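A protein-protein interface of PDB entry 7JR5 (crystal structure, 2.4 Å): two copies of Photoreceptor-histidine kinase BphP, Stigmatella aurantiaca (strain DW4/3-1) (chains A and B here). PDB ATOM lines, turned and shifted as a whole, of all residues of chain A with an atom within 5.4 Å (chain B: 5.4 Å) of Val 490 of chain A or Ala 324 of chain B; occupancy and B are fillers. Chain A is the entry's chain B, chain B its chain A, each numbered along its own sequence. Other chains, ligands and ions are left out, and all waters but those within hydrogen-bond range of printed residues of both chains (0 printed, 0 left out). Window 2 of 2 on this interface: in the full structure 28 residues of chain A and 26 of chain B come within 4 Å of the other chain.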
ATOM      1  N   LEU A 416      10.927 -25.541 -20.765  1.00  0.00           N
ATOM      2  CA  LEU A 416      11.477 -24.186 -21.043  1.00  0.00           C
ATOM      3  C   LEU A 416      12.477 -24.248 -22.213  1.00  0.00           C
ATOM      4  O   LEU A 416      12.905 -23.166 -22.654  1.00  0.00           O
ATOM      5  CB  LEU A 416      12.138 -23.644 -19.771  1.00  0.00           C
ATOM      6  CG  LEU A 416      11.953 -22.153 -19.471  1.00  0.00           C
ATOM      7  CD1 LEU A 416      12.609 -21.268 -20.511  1.00  0.00           C
ATOM      8  CD2 LEU A 416      10.484 -21.807 -19.334  1.00  0.00           C
ATOM      9  N   PHE A 485       3.827 -17.782 -20.079  1.00  0.00           N
ATOM     10  CA  PHE A 485       4.921 -17.810 -19.078  1.00  0.00           C
ATOM     11  C   PHE A 485       6.131 -18.571 -19.655  1.00  0.00           C
ATOM     12  O   PHE A 485       7.280 -18.221 -19.245  1.00  0.00           O
ATOM     13  CB  PHE A 485       4.375 -18.432 -17.798  1.00  0.00           C
ATOM     14  CG  PHE A 485       5.112 -18.095 -16.533  1.00  0.00           C
ATOM     15  CD1 PHE A 485       6.234 -18.811 -16.140  1.00  0.00           C
ATOM     16  CD2 PHE A 485       4.659 -17.083 -15.699  1.00  0.00           C
ATOM     17  CE1 PHE A 485       6.889 -18.501 -14.954  1.00  0.00           C
ATOM     18  CE2 PHE A 485       5.315 -16.784 -14.515  1.00  0.00           C
ATOM     19  CZ  PHE A 485       6.422 -17.498 -14.138  1.00  0.00           C
ATOM     20  N   ARG A 486       5.917 -19.550 -20.554  1.00  0.00           N
ATOM     21  CA  ARG A 486       6.969 -20.006 -21.514  1.00  0.00           C
ATOM     22  C   ARG A 486       7.776 -18.771 -21.930  1.00  0.00           C
ATOM     23  O   ARG A 486       8.969 -18.703 -21.565  1.00  0.00           O
ATOM     24  CB  ARG A 486       6.416 -20.609 -22.813  1.00  0.00           C
ATOM     25  CG  ARG A 486       5.956 -22.057 -22.732  1.00  0.00           C
ATOM     26  CD  ARG A 486       6.749 -23.005 -23.615  1.00  0.00           C
ATOM     27  NE  ARG A 486       6.335 -23.006 -25.017  1.00  0.00           N
ATOM     28  CZ  ARG A 486       6.787 -22.190 -25.956  1.00  0.00           C
ATOM     29  NH1 ARG A 486       7.664 -21.258 -25.649  1.00  0.00           N
ATOM     30  NH2 ARG A 486       6.360 -22.295 -27.203  1.00  0.00           N
ATOM     31  N   GLY A 487       7.120 -17.825 -22.625  1.00  0.00           N
ATOM     32  CA  GLY A 487       7.746 -16.661 -23.294  1.00  0.00           C
ATOM     33  C   GLY A 487       8.414 -15.722 -22.304  1.00  0.00           C
ATOM     34  O   GLY A 487       9.491 -15.174 -22.614  1.00  0.00           O
ATOM     35  N   ALA A 488       7.803 -15.548 -21.134  1.00  0.00           N
ATOM     36  CA  ALA A 488       8.360 -14.768 -20.009  1.00  0.00           C
ATOM     37  C   ALA A 488       9.833 -15.154 -19.821  1.00  0.00           C
ATOM     38  O   ALA A 488      10.727 -14.286 -20.017  1.00  0.00           O
ATOM     39  CB  ALA A 488       7.538 -15.024 -18.774  1.00  0.00           C
ATOM     40  N   LEU A 489      10.059 -16.438 -19.536  1.00  0.00           N
ATOM     41  CA  LEU A 489      11.352 -17.009 -19.077  1.00  0.00           C
ATOM     42  C   LEU A 489      12.322 -17.157 -20.253  1.00  0.00           C
ATOM     43  O   LEU A 489      13.408 -16.539 -20.181  1.00  0.00           O
ATOM     44  CB  LEU A 489      11.067 -18.354 -18.413  1.00  0.00           C
ATOM     45  CG  LEU A 489      10.716 -18.274 -16.936  1.00  0.00           C
ATOM     46  CD1 LEU A 489       9.821 -17.067 -16.638  1.00  0.00           C
ATOM     47  CD2 LEU A 489      10.075 -19.566 -16.461  1.00  0.00           C
ATOM     48  N   VAL A 490      11.946 -17.939 -21.274  1.00  0.00           N
ATOM     49  CA  VAL A 490      12.829 -18.367 -22.403  1.00  0.00           C
ATOM     50  C   VAL A 490      14.284 -17.939 -22.122  1.00  0.00           C
ATOM     51  O   VAL A 490      14.652 -16.775 -21.978  1.00  0.00           O
ATOM     52  CB  VAL A 490      12.321 -17.840 -23.757  1.00  0.00           C
ATOM     53  CG1 VAL A 490      11.047 -18.551 -24.192  1.00  0.00           C
ATOM     54  CG2 VAL A 490      12.110 -16.331 -23.749  1.00  0.00           C
ATOM     55  N   LEU B 320       2.299 -17.139 -30.831  1.00  0.00           N
ATOM     56  CA  LEU B 320       3.249 -16.912 -29.708  1.00  0.00           C
ATOM     57  C   LEU B 320       4.151 -18.130 -29.484  1.00  0.00           C
ATOM     58  O   LEU B 320       5.384 -17.965 -29.481  1.00  0.00           O
ATOM     59  CB  LEU B 320       2.442 -16.668 -28.438  1.00  0.00           C
ATOM     60  CG  LEU B 320       3.286 -16.399 -27.201  1.00  0.00           C
ATOM     61  CD1 LEU B 320       3.746 -14.958 -27.214  1.00  0.00           C
ATOM     62  CD2 LEU B 320       2.504 -16.702 -25.938  1.00  0.00           C
ATOM     63  N   GLY B 321       3.550 -19.291 -29.236  1.00  0.00           N
ATOM     64  CA  GLY B 321       4.280 -20.548 -29.028  1.00  0.00           C
ATOM     65  C   GLY B 321       5.370 -20.672 -30.062  1.00  0.00           C
ATOM     66  O   GLY B 321       6.549 -20.746 -29.663  1.00  0.00           O
ATOM     67  N   GLN B 322       4.976 -20.694 -31.340  1.00  0.00           N
ATOM     68  CA  GLN B 322       5.917 -20.655 -32.494  1.00  0.00           C
ATOM     69  C   GLN B 322       7.062 -19.717 -32.093  1.00  0.00           C
ATOM     70  O   GLN B 322       8.213 -20.169 -32.082  1.00  0.00           O
ATOM     71  CB  GLN B 322       5.222 -20.174 -33.774  1.00  0.00           C
ATOM     72  CG  GLN B 322       4.899 -21.274 -34.779  1.00  0.00           C
ATOM     73  CD  GLN B 322       3.591 -21.026 -35.500  1.00  0.00           C
ATOM     74  OE1 GLN B 322       2.677 -21.839 -35.451  1.00  0.00           O
ATOM     75  NE2 GLN B 322       3.466 -19.887 -36.162  1.00  0.00           N
ATOM     76  N   LEU B 323       6.694 -18.498 -31.676  1.00  0.00           N
ATOM     77  CA  LEU B 323       7.559 -17.301 -31.525  1.00  0.00           C
ATOM     78  C   LEU B 323       8.615 -17.585 -30.437  1.00  0.00           C
ATOM     79  O   LEU B 323       9.818 -17.698 -30.790  1.00  0.00           O
ATOM     80  CB  LEU B 323       6.639 -16.102 -31.241  1.00  0.00           C
ATOM     81  CG  LEU B 323       7.124 -14.702 -31.631  1.00  0.00           C
ATOM     82  CD1 LEU B 323       7.324 -13.848 -30.390  1.00  0.00           C
ATOM     83  CD2 LEU B 323       8.388 -14.719 -32.489  1.00  0.00           C
ATOM     84  N   ALA B 324       8.187 -17.822 -29.194  1.00  0.00           N
ATOM     85  CA  ALA B 324       9.040 -18.075 -27.997  1.00  0.00           C
ATOM     86  C   ALA B 324      10.074 -19.214 -28.179  1.00  0.00           C
ATOM     87  O   ALA B 324      11.080 -19.252 -27.430  1.00  0.00           O
ATOM     88  CB  ALA B 324       8.144 -18.375 -26.824  1.00  0.00           C
ATOM     89  N   THR B 325       9.829 -20.166 -29.076  1.00  0.00           N
ATOM     90  CA  THR B 325      10.733 -21.318 -29.314  1.00  0.00           C
ATOM     91  C   THR B 325      11.536 -21.080 -30.596  1.00  0.00           C
ATOM     92  O   THR B 325      12.199 -22.045 -31.073  1.00  0.00           O
ATOM     93  CB  THR B 325       9.949 -22.633 -29.272  1.00  0.00           C
ATOM     94  OG1 THR B 325       8.791 -22.530 -30.100  1.00  0.00           O
ATOM     95  CG2 THR B 325       9.552 -22.967 -27.853  1.00  0.00           C
ATOM     96  N   ALA B 326      11.486 -19.846 -31.108  1.00  0.00           N
ATOM     97  CA  ALA B 326      12.601 -19.198 -31.824  1.00  0.00           C
ATOM     98  C   ALA B 326      13.431 -18.464 -30.768  1.00  0.00           C
ATOM     99  O   ALA B 326      14.635 -18.750 -30.658  1.00  0.00           O
ATOM    100  CB  ALA B 326      12.076 -18.259 -32.874  1.00  0.00           C
ATOM    101  N   MET B 327      12.752 -17.602 -30.000  1.00  0.00           N
ATOM    102  CA  MET B 327      13.230 -16.762 -28.857  1.00  0.00           C
ATOM    103  C   MET B 327      14.151 -17.514 -27.895  1.00  0.00           C
ATOM    104  O   MET B 327      15.037 -16.842 -27.345  1.00  0.00           O
ATOM    105  CB  MET B 327      12.032 -16.290 -28.026  1.00  0.00           C
ATOM    106  CG  MET B 327      12.117 -14.860 -27.527  1.00  0.00           C
ATOM    107  SD  MET B 327      11.367 -13.706 -28.701  1.00  0.00           S
ATOM    108  CE  MET B 327      11.450 -12.217 -27.713  1.00  0.00           C
ATOM    109  N   GLY B 328      13.877 -18.800 -27.621  1.00  0.00           N
ATOM    110  CA  GLY B 328      14.682 -19.678 -26.740  1.00  0.00           C
ATOM    111  C   GLY B 328      15.350 -20.811 -27.514  1.00  0.00           C
ATOM    112  O   GLY B 328      14.915 -21.994 -27.344  1.00  0.00           O
ATOM    113  N   ALA B 488       7.948 -10.648 -22.067  1.00  0.00           N
ATOM    114  CA  ALA B 488       8.931 -11.346 -22.926  1.00  0.00           C
ATOM    115  C   ALA B 488      10.252 -10.569 -22.993  1.00  0.00           C
ATOM    116  O   ALA B 488      11.301 -11.225 -22.918  1.00  0.00           O
ATOM    117  CB  ALA B 488       8.356 -11.576 -24.302  1.00  0.00           C
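1 position is printed for both chains.
Val 490 of chain A touches just one residue of chain B: Ala 324. Ala 324 of chain B touches just these residues of chain A: Arg 486 (3.2 Å), Gly 487 (3.9 Å) and Val 490 (3.3 Å). Of the printed residues of chain A, Ala 488 of chain B touches Gly 487. Of the printed residues of chain A, Gly 321 of chain B touches Arg 486 (2.9 Å). Ala 488 of chain A touches none of the printed residues of chain B. The nearest residue of chain B that does not touch Val 490 of chain A is Met 327 of chain B (4.1 Å). The nearest printed residue of chain A that does not touch Ala 488 of chain B is Ala 488 of chain A (4.3 Å).
CB of Ala 324 of chain B touches NH1 of Arg 486 of chain A, at 3.2 Å. Arg 486 of chain A touches Thr 325 of chain B (NH2 to CG2, 3.3 Å). Gly 487 of chain A touches Ala 324 of chain B. Gly 487 of chain A touches Ala 488 of chain B (O to CA, 3.9 Å). Val 490 of chain A touches Ala 324 of chain B.
Of the 7 printed residues of chain A, 3 touch a printed residue of chain B. Hydrophobic or aromatic side chains of chain A that line the printed part of chain B: Val 490. Along chain A the printed residues that touch a printed residue of chain B span positions 486 to 490. Hydrophobic or aromatic side chains of chain B that line the printed part of chain A: Ala 324.
The backbone carbonyl oxygen (O) of Gly 321 of chain B is in hydrogen-bond range of the guanidinium group (NH2) of Arg 486 of chain A (2.9 Å).
The backbone carbonyl oxygen of Gln 322 of chain B is in hydrogen-bond range of the side-chain hydroxyl of Thr 325 of chain B (3.1 Å). The backbone carbonyl oxygen (O) of Gly 321 of chain B is in hydrogen-bond range of the side-chain hydroxyl (OG1) of Thr 325 of chain B, 2.9 Å away.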
